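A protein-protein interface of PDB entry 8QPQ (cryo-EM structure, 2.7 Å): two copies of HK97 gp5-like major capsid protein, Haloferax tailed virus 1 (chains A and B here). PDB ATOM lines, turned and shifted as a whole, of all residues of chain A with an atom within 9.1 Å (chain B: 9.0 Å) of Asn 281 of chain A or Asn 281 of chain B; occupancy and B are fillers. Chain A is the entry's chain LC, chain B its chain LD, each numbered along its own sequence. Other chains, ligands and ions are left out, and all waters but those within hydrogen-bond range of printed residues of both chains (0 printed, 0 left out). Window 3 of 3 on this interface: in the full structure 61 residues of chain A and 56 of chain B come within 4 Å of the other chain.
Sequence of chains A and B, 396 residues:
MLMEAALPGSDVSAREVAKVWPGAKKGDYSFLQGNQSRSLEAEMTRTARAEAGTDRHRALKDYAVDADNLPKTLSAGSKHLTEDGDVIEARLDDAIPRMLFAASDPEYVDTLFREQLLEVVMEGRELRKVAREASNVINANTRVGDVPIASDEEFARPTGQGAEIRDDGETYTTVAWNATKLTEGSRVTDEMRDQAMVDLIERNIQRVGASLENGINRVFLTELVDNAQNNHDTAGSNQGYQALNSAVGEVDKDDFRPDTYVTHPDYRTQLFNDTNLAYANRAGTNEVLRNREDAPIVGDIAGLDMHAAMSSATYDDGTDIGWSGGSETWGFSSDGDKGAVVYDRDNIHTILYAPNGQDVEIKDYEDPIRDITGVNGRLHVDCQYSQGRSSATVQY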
ATOM      1  N   THR A 275      -1.964  -1.089   6.487  1.00  0.00           N
ATOM      2  CA  THR A 275      -2.506  -0.158   5.502  1.00  0.00           C
ATOM      3  C   THR A 275      -3.873   0.377   5.911  1.00  0.00           C
ATOM      4  O   THR A 275      -4.196   1.506   5.577  1.00  0.00           O
ATOM      5  CB  THR A 275      -2.551  -0.742   4.095  1.00  0.00           C
ATOM      6  OG1 THR A 275      -3.459  -1.842   4.140  1.00  0.00           O
ATOM      7  CG2 THR A 275      -1.182  -1.163   3.614  1.00  0.00           C
ATOM      8  N   ASN A 276      -4.637  -0.363   6.710  1.00  0.00           N
ATOM      9  CA  ASN A 276      -5.932   0.091   7.198  1.00  0.00           C
ATOM     10  C   ASN A 276      -5.819   1.302   8.137  1.00  0.00           C
ATOM     11  O   ASN A 276      -6.781   2.051   8.263  1.00  0.00           O
ATOM     12  CB  ASN A 276      -6.688  -1.068   7.846  1.00  0.00           C
ATOM     13  CG  ASN A 276      -8.192  -0.876   7.794  1.00  0.00           C
ATOM     14  OD1 ASN A 276      -8.713   0.007   7.107  1.00  0.00           O
ATOM     15  ND2 ASN A 276      -8.902  -1.694   8.539  1.00  0.00           N
ATOM     16  N   LEU A 277      -4.660   1.493   8.791  1.00  0.00           N
ATOM     17  CA  LEU A 277      -4.402   2.621   9.677  1.00  0.00           C
ATOM     18  C   LEU A 277      -3.460   3.641   9.027  1.00  0.00           C
ATOM     19  O   LEU A 277      -3.651   4.846   9.188  1.00  0.00           O
ATOM     20  CB  LEU A 277      -3.839   2.092  10.995  1.00  0.00           C
ATOM     21  CG  LEU A 277      -4.827   1.681  12.076  1.00  0.00           C
ATOM     22  CD1 LEU A 277      -5.608   0.447  11.695  1.00  0.00           C
ATOM     23  CD2 LEU A 277      -4.043   1.373  13.337  1.00  0.00           C
ATOM     24  N   ALA A 278      -2.432   3.164   8.311  1.00  0.00           N
ATOM     25  CA  ALA A 278      -1.412   3.989   7.686  1.00  0.00           C
ATOM     26  C   ALA A 278      -1.958   4.830   6.530  1.00  0.00           C
ATOM     27  O   ALA A 278      -1.519   5.950   6.315  1.00  0.00           O
ATOM     28  CB  ALA A 278      -0.280   3.101   7.239  1.00  0.00           C
ATOM     29  N   TYR A 279      -2.910   4.297   5.758  1.00  0.00           N
ATOM     30  CA  TYR A 279      -3.529   5.038   4.669  1.00  0.00           C
ATOM     31  C   TYR A 279      -4.699   5.838   5.231  1.00  0.00           C
ATOM     32  O   TYR A 279      -5.673   5.247   5.692  1.00  0.00           O
ATOM     33  CB  TYR A 279      -4.016   4.090   3.563  1.00  0.00           C
ATOM     34  CG  TYR A 279      -3.000   3.249   2.821  1.00  0.00           C
ATOM     35  CD1 TYR A 279      -1.630   3.327   3.071  1.00  0.00           C
ATOM     36  CD2 TYR A 279      -3.425   2.365   1.837  1.00  0.00           C
ATOM     37  CE1 TYR A 279      -0.727   2.527   2.382  1.00  0.00           C
ATOM     38  CE2 TYR A 279      -2.535   1.564   1.137  1.00  0.00           C
ATOM     39  CZ  TYR A 279      -1.178   1.644   1.413  1.00  0.00           C
ATOM     40  OH  TYR A 279      -0.283   0.887   0.707  1.00  0.00           O
ATOM     41  N   ALA A 280      -4.647   7.166   5.091  1.00  0.00           N
ATOM     42  CA  ALA A 280      -5.678   8.068   5.599  1.00  0.00           C
ATOM     43  C   ALA A 280      -7.063   7.727   5.057  1.00  0.00           C
ATOM     44  O   ALA A 280      -8.054   7.705   5.777  1.00  0.00           O
ATOM     45  CB  ALA A 280      -5.301   9.491   5.299  1.00  0.00           C
ATOM     46  N   ASN A 281      -7.111   7.401   3.760  1.00  0.00           N
ATOM     47  CA  ASN A 281      -8.184   6.796   2.985  1.00  0.00           C
ATOM     48  C   ASN A 281      -8.912   5.681   3.770  1.00  0.00           C
ATOM     49  O   ASN A 281     -10.120   5.716   3.956  1.00  0.00           O
ATOM     50  CB  ASN A 281      -7.465   6.289   1.723  1.00  0.00           C
ATOM     51  CG  ASN A 281      -8.343   5.703   0.660  1.00  0.00           C
ATOM     52  OD1 ASN A 281      -9.420   6.227   0.394  1.00  0.00           O
ATOM     53  ND2 ASN A 281      -7.886   4.605   0.088  1.00  0.00           N
ATOM     54  N   ARG A 282      -8.146   4.692   4.229  1.00  0.00           N
ATOM     55  CA  ARG A 282      -8.655   3.480   4.850  1.00  0.00           C
ATOM     56  C   ARG A 282      -8.984   3.705   6.321  1.00  0.00           C
ATOM     57  O   ARG A 282      -9.937   3.124   6.834  1.00  0.00           O
ATOM     58  CB  ARG A 282      -7.698   2.308   4.621  1.00  0.00           C
ATOM     59  CG  ARG A 282      -7.502   2.006   3.126  1.00  0.00           C
ATOM     60  CD  ARG A 282      -6.641   0.792   2.900  1.00  0.00           C
ATOM     61  NE  ARG A 282      -6.471   0.558   1.468  1.00  0.00           N
ATOM     62  CZ  ARG A 282      -5.748  -0.409   0.915  1.00  0.00           C
ATOM     63  NH1 ARG A 282      -5.656  -0.486  -0.400  1.00  0.00           N
ATOM     64  NH2 ARG A 282      -5.007  -1.208   1.661  1.00  0.00           N
ATOM     65  N   ALA A 283      -8.246   4.580   7.014  1.00  0.00           N
ATOM     66  CA  ALA A 283      -8.482   4.926   8.414  1.00  0.00           C
ATOM     67  C   ALA A 283      -9.598   5.954   8.621  1.00  0.00           C
ATOM     68  O   ALA A 283     -10.099   6.103   9.731  1.00  0.00           O
ATOM     69  CB  ALA A 283      -7.185   5.407   8.999  1.00  0.00           C
ATOM     70  N   GLY A 284      -9.928   6.735   7.583  1.00  0.00           N
ATOM     71  CA  GLY A 284     -10.796   7.904   7.700  1.00  0.00           C
ATOM     72  C   GLY A 284     -10.116   9.135   8.304  1.00  0.00           C
ATOM     73  O   GLY A 284     -10.789  10.147   8.496  1.00  0.00           O
ATOM     74  N   THR A 285      -8.826   9.028   8.650  1.00  0.00           N
ATOM     75  CA  THR A 285      -8.025  10.072   9.269  1.00  0.00           C
ATOM     76  C   THR A 285      -6.543   9.834   8.989  1.00  0.00           C
ATOM     77  O   THR A 285      -6.109   8.698   8.911  1.00  0.00           O
ATOM     78  CB  THR A 285      -8.292  10.141  10.778  1.00  0.00           C
ATOM     79  OG1 THR A 285      -7.672  11.348  11.198  1.00  0.00           O
ATOM     80  CG2 THR A 285      -7.852   8.922  11.573  1.00  0.00           C
ATOM     81  N   ASN A 286      -5.744  10.897   8.855  1.00  0.00           N
ATOM     82  CA  ASN A 286      -4.295  10.765   8.698  1.00  0.00           C
ATOM     83  C   ASN A 286      -3.543  10.779  10.034  1.00  0.00           C
ATOM     84  O   ASN A 286      -2.306  10.802  10.050  1.00  0.00           O
ATOM     85  CB  ASN A 286      -3.713  11.758   7.687  1.00  0.00           C
ATOM     86  CG  ASN A 286      -3.781  13.227   8.068  1.00  0.00           C
ATOM     87  OD1 ASN A 286      -4.412  13.610   9.052  1.00  0.00           O
ATOM     88  ND2 ASN A 286      -3.077  14.051   7.316  1.00  0.00           N
ATOM     89  N   GLU A 287      -4.248  10.728  11.163  1.00  0.00           N
ATOM     90  CA  GLU A 287      -3.676  10.856  12.497  1.00  0.00           C
ATOM     91  C   GLU A 287      -2.627   9.790  12.817  1.00  0.00           C
ATOM     92  O   GLU A 287      -1.645  10.081  13.488  1.00  0.00           O
ATOM     93  CB  GLU A 287      -4.780  10.898  13.549  1.00  0.00           C
ATOM     94  CG  GLU A 287      -5.623  12.137  13.569  1.00  0.00           C
ATOM     95  CD  GLU A 287      -4.965  13.392  14.077  1.00  0.00           C
ATOM     96  OE1 GLU A 287      -4.621  13.380  15.259  1.00  0.00           O
ATOM     97  OE2 GLU A 287      -4.733  14.304  13.251  1.00  0.00           O
ATOM     98  N   LEU A 289      -0.696   8.142  10.505  1.00  0.00           N
ATOM     99  CA  LEU A 289       0.411   8.483   9.626  1.00  0.00           C
ATOM    100  C   LEU A 289       1.229   9.639  10.209  1.00  0.00           C
ATOM    101  O   LEU A 289       2.464   9.591  10.187  1.00  0.00           O
ATOM    102  CB  LEU A 289      -0.157   8.840   8.252  1.00  0.00           C
ATOM    103  CG  LEU A 289       0.837   9.294   7.196  1.00  0.00           C
ATOM    104  CD1 LEU A 289       1.839   8.198   6.881  1.00  0.00           C
ATOM    105  CD2 LEU A 289       0.089   9.677   5.930  1.00  0.00           C
ATOM    106  N   THR B 275       3.755   5.795  -2.013  1.00  0.00           N
ATOM    107  CA  THR B 275       2.331   5.978  -2.298  1.00  0.00           C
ATOM    108  C   THR B 275       1.561   6.440  -1.063  1.00  0.00           C
ATOM    109  O   THR B 275       0.577   7.140  -1.204  1.00  0.00           O
ATOM    110  CB  THR B 275       1.694   4.727  -2.898  1.00  0.00           C
ATOM    111  OG1 THR B 275       1.644   3.711  -1.900  1.00  0.00           O
ATOM    112  CG2 THR B 275       2.416   4.239  -4.130  1.00  0.00           C
ATOM    113  N   ASN B 276       2.025   6.131   0.141  1.00  0.00           N
ATOM    114  CA  ASN B 276       1.411   6.593   1.379  1.00  0.00           C
ATOM    115  C   ASN B 276       1.454   8.119   1.538  1.00  0.00           C
ATOM    116  O   ASN B 276       0.619   8.684   2.238  1.00  0.00           O
ATOM    117  CB  ASN B 276       2.055   5.903   2.582  1.00  0.00           C
ATOM    118  CG  ASN B 276       1.101   5.702   3.743  1.00  0.00           C
ATOM    119  OD1 ASN B 276       1.223   4.698   4.441  1.00  0.00           O
ATOM    120  ND2 ASN B 276       0.130   6.566   3.990  1.00  0.00           N
ATOM    121  N   LEU B 277       2.404   8.803   0.878  1.00  0.00           N
ATOM    122  CA  LEU B 277       2.589  10.247   0.960  1.00  0.00           C
ATOM    123  C   LEU B 277       2.284  10.935  -0.367  1.00  0.00           C
ATOM    124  O   LEU B 277       1.697  12.012  -0.390  1.00  0.00           O
ATOM    125  CB  LEU B 277       4.008  10.555   1.448  1.00  0.00           C
ATOM    126  CG  LEU B 277       4.218  10.167   2.915  1.00  0.00           C
ATOM    127  CD1 LEU B 277       5.690  10.282   3.258  1.00  0.00           C
ATOM    128  CD2 LEU B 277       3.400  11.028   3.874  1.00  0.00           C
ATOM    129  N   ALA B 278       2.668  10.314  -1.482  1.00  0.00           N
ATOM    130  CA  ALA B 278       2.471  10.833  -2.836  1.00  0.00           C
ATOM    131  C   ALA B 278       0.995  10.838  -3.235  1.00  0.00           C
ATOM    132  O   ALA B 278       0.555  11.760  -3.921  1.00  0.00           O
ATOM    133  CB  ALA B 278       3.264  10.001  -3.812  1.00  0.00           C
ATOM    134  N   TYR B 279       0.211   9.835  -2.801  1.00  0.00           N
ATOM    135  CA  TYR B 279      -1.204   9.800  -3.119  1.00  0.00           C
ATOM    136  C   TYR B 279      -1.962  10.574  -2.044  1.00  0.00           C
ATOM    137  O   TYR B 279      -1.956  10.182  -0.875  1.00  0.00           O
ATOM    138  CB  TYR B 279      -1.727   8.365  -3.179  1.00  0.00           C
ATOM    139  CG  TYR B 279      -1.148   7.388  -4.176  1.00  0.00           C
ATOM    140  CD1 TYR B 279      -0.204   7.767  -5.123  1.00  0.00           C
ATOM    141  CD2 TYR B 279      -1.620   6.081  -4.208  1.00  0.00           C
ATOM    142  CE1 TYR B 279       0.248   6.866  -6.085  1.00  0.00           C
ATOM    143  CE2 TYR B 279      -1.171   5.170  -5.155  1.00  0.00           C
ATOM    144  CZ  TYR B 279      -0.231   5.565  -6.098  1.00  0.00           C
ATOM    145  OH  TYR B 279       0.222   4.683  -7.041  1.00  0.00           O
ATOM    146  N   ALA B 280      -2.660  11.649  -2.453  1.00  0.00           N
ATOM    147  CA  ALA B 280      -3.407  12.510  -1.542  1.00  0.00           C
ATOM    148  C   ALA B 280      -4.401  11.725  -0.688  1.00  0.00           C
ATOM    149  O   ALA B 280      -4.535  11.944   0.503  1.00  0.00           O
ATOM    150  CB  ALA B 280      -4.108  13.579  -2.326  1.00  0.00           C
ATOM    151  N   ASN B 281      -5.061  10.744  -1.312  1.00  0.00           N
ATOM    152  CA  ASN B 281      -5.838   9.656  -0.762  1.00  0.00           C
ATOM    153  C   ASN B 281      -5.225   9.036   0.506  1.00  0.00           C
ATOM    154  O   ASN B 281      -5.783   9.115   1.608  1.00  0.00           O
ATOM    155  CB  ASN B 281      -5.950   8.649  -1.914  1.00  0.00           C
ATOM    156  CG  ASN B 281      -7.080   7.680  -1.802  1.00  0.00           C
ATOM    157  OD1 ASN B 281      -8.150   8.013  -1.300  1.00  0.00           O
ATOM    158  ND2 ASN B 281      -6.852   6.500  -2.333  1.00  0.00           N
ATOM    159  N   ARG B 282      -4.008   8.500   0.358  1.00  0.00           N
ATOM    160  CA  ARG B 282      -3.314   7.770   1.405  1.00  0.00           C
ATOM    161  C   ARG B 282      -2.719   8.707   2.458  1.00  0.00           C
ATOM    162  O   ARG B 282      -2.621   8.332   3.630  1.00  0.00           O
ATOM    163  CB  ARG B 282      -2.264   6.829   0.805  1.00  0.00           C
ATOM    164  CG  ARG B 282      -2.733   5.837  -0.231  1.00  0.00           C
ATOM    165  CD  ARG B 282      -1.668   4.735  -0.367  1.00  0.00           C
ATOM    166  NE  ARG B 282      -1.568   3.821  -1.490  1.00  0.00           N
ATOM    167  CZ  ARG B 282      -2.541   3.133  -2.074  1.00  0.00           C
ATOM    168  NH1 ARG B 282      -2.267   2.256  -3.021  1.00  0.00           N
ATOM    169  NH2 ARG B 282      -3.787   3.279  -1.661  1.00  0.00           N
ATOM    170  N   ALA B 283      -2.340   9.931   2.075  1.00  0.00           N
ATOM    171  CA  ALA B 283      -1.775  10.931   2.973  1.00  0.00           C
ATOM    172  C   ALA B 283      -2.826  11.766   3.713  1.00  0.00           C
ATOM    173  O   ALA B 283      -2.496  12.486   4.666  1.00  0.00           O
ATOM    174  CB  ALA B 283      -0.877  11.816   2.151  1.00  0.00           C
ATOM    175  N   GLY B 284      -4.075  11.781   3.229  1.00  0.00           N
ATOM    176  CA  GLY B 284      -5.130  12.669   3.711  1.00  0.00           C
ATOM    177  C   GLY B 284      -4.989  14.132   3.251  1.00  0.00           C
ATOM    178  O   GLY B 284      -5.627  15.002   3.826  1.00  0.00           O
ATOM    179  N   THR B 285      -4.053  14.388   2.321  1.00  0.00           N
ATOM    180  CA  THR B 285      -3.449  15.692   2.037  1.00  0.00           C
ATOM    181  C   THR B 285      -2.703  15.601   0.703  1.00  0.00           C
ATOM    182  O   THR B 285      -1.888  14.714   0.583  1.00  0.00           O
ATOM    183  CB  THR B 285      -2.565  16.070   3.265  1.00  0.00           C
ATOM    184  OG1 THR B 285      -3.476  16.701   4.172  1.00  0.00           O
ATOM    185  CG2 THR B 285      -1.307  16.869   3.056  1.00  0.00           C
ATOM    186  N   ASN B 286      -2.877  16.537  -0.255  1.00  0.00           N
ATOM    187  CA  ASN B 286      -2.042  16.549  -1.454  1.00  0.00           C
ATOM    188  C   ASN B 286      -0.738  17.349  -1.309  1.00  0.00           C
ATOM    189  O   ASN B 286      -0.007  17.504  -2.270  1.00  0.00           O
ATOM    190  CB  ASN B 286      -2.813  16.943  -2.719  1.00  0.00           C
ATOM    191  CG  ASN B 286      -3.332  18.360  -2.780  1.00  0.00           C
ATOM    192  OD1 ASN B 286      -3.217  19.136  -1.835  1.00  0.00           O
ATOM    193  ND2 ASN B 286      -3.841  18.734  -3.940  1.00  0.00           N
ATOM    194  N   GLU B 287      -0.431  17.809  -0.098  1.00  0.00           N
ATOM    195  CA  GLU B 287       0.654  18.765   0.136  1.00  0.00           C
ATOM    196  C   GLU B 287       2.031  18.179  -0.193  1.00  0.00           C
ATOM    197  O   GLU B 287       2.896  18.929  -0.610  1.00  0.00           O
ATOM    198  CB  GLU B 287       0.592  19.277   1.571  1.00  0.00           C
ATOM    199  CG  GLU B 287       1.218  20.638   1.636  1.00  0.00           C
ATOM    200  CD  GLU B 287       0.333  21.821   1.361  1.00  0.00           C
ATOM    201  OE1 GLU B 287      -0.913  21.701   1.310  1.00  0.00           O
ATOM    202  OE2 GLU B 287       0.924  22.889   1.138  1.00  0.00           O
ATOM    203  N   LEU B 289       2.643  15.878  -2.697  1.00  0.00           N
ATOM    204  CA  LEU B 289       2.625  15.917  -4.160  1.00  0.00           C
ATOM    205  C   LEU B 289       2.867  17.351  -4.655  1.00  0.00           C
ATOM    206  O   LEU B 289       3.628  17.590  -5.578  1.00  0.00           O
ATOM    207  CB  LEU B 289       1.274  15.369  -4.629  1.00  0.00           C
ATOM    208  CG  LEU B 289       1.104  14.899  -6.070  1.00  0.00           C
ATOM    209  CD1 LEU B 289      -0.337  14.483  -6.272  1.00  0.00           C
ATOM    210  CD2 LEU B 289       1.431  15.942  -7.123  1.00  0.00           C
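Tyr 279 of chain A touches Asn 276 of chain B, but with the chains exchanged Asn 276 of chain A does not touch Tyr 279 of chain B (13.0 Å).
Tyr 279 of chain A touches Arg 282 of chain B, but with the chains exchanged Arg 282 of chain A does not touch Tyr 279 of chain B (8.6 Å).
Ala 280 of chain A touches Ala 283 of chain B, but with the chains exchanged Ala 283 of chain A does not touch Ala 280 of chain B (10.5 Å).
Leu 289 of chain A touches Asn 276 of chain B, but with the chains exchanged Asn 276 of chain A does not touch Leu 289 of chain B (20.0 Å).
14 positions are printed for both chains.
Of the 13 pairs that touch across the chains among the printed residues, 1 has its exchanged pair printed and touching as well.
The side-chain amide nitrogen (ND2) of Asn 286 of chain A lies within hydrogen-bond range of the backbone carbonyl oxygen (O) of Ala 283 of chain B (3.1 Å).
The side-chain amide nitrogen of Asn 276 of chain B is in hydrogen-bond range of the backbone carbonyl oxygen of Ala 278 of chain A (2.9 Å).
The backbone NH of Ala 280 of chain A is in hydrogen-bond range of the backbone carbonyl oxygen of Arg 282 of chain B, 2.8 Å away.
The side-chain amide oxygen (OD1) of Asn 281 of chain A sits close to the side-chain amide oxygen (OD1) of Asn 281 of chain B (2.8 Å).
Of chain B, only Asn 281 (2.8 Å) comes within 4 Å of Asn 281 of chain A.
Of the printed residues of chain B, Leu 289 of chain A touches Asn 276, Arg 282 and Ala 283.
Printed residues of chain B within 4 Å of Tyr 279 of chain A: Asn 276 (3.4 Å) and Arg 282 (3.5 Å).
Leu 289 of chain B touches none of the printed residues of chain A.
Ala 278 of chain B touches none of the printed residues of chain A.
The nearest residue of chain B that does not touch Asn 281 of chain A is Arg 282 of chain B (4.3 Å).
The nearest residue of chain A that does not touch Asn 281 of chain B is Tyr 279 of chain A (5.0 Å).
The nearest printed residue of chain B that does not touch Leu 289 of chain A is Leu 277 of chain B (4.1 Å).
Among the printed residues, pairs that only touch across the chains: Ala 280 of chain A with Gly 284 of chain B, Tyr 279 of chain A with Asn 276 of chain B, Tyr 279 of chain A with Arg 282 of chain B, Leu 289 of chain A with Asn 276 of chain B, Leu 289 of chain A with Ala 283 of chain B, Ala 280 of chain A with Ala 283 of chain B, Ala 280 of chain A with Asn 281 of chain B, Ala 278 of chain A with Arg 282 of chain B and Leu 289 of chain A with Arg 282 of chain B.
Printed residues of chain B that touch a printed residue of chain A: Asn 276, Asn 281, Arg 282, Ala 283 and Gly 284.
Printed residues of chain A that touch a printed residue of chain B: Ala 278, Tyr 279, Ala 280, Asn 281, Asn 286 and Leu 289.
Along chain A the printed residues that touch a printed residue of chain B span positions 278 to 289.
Among the printed residues, 13 pairs touch across the chains.
Among the printed residues, no Asp or Glu carboxylate lies within 4 Å of a Lys or Arg side-chain nitrogen of the other chain.
O of Asn 276 of chain B lies within hydrogen-bond range of N of Ala 283 of chain B, 3.2 Å away.
The backbone carbonyl oxygen (O) of Arg 282 of chain B is in hydrogen-bond range of the side-chain amide nitrogen (ND2) of Asn 276 of chain B, at 3.3 Å.
The backbone carbonyl oxygen (O) of Ala 280 of chain A lies within hydrogen-bond range of the backbone NH (N) of Thr 285 of chain A (3.3 Å).
OG1 of Thr 275 of chain B is in hydrogen-bond range of NE of Arg 282 of chain B, 3.2 Å away.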
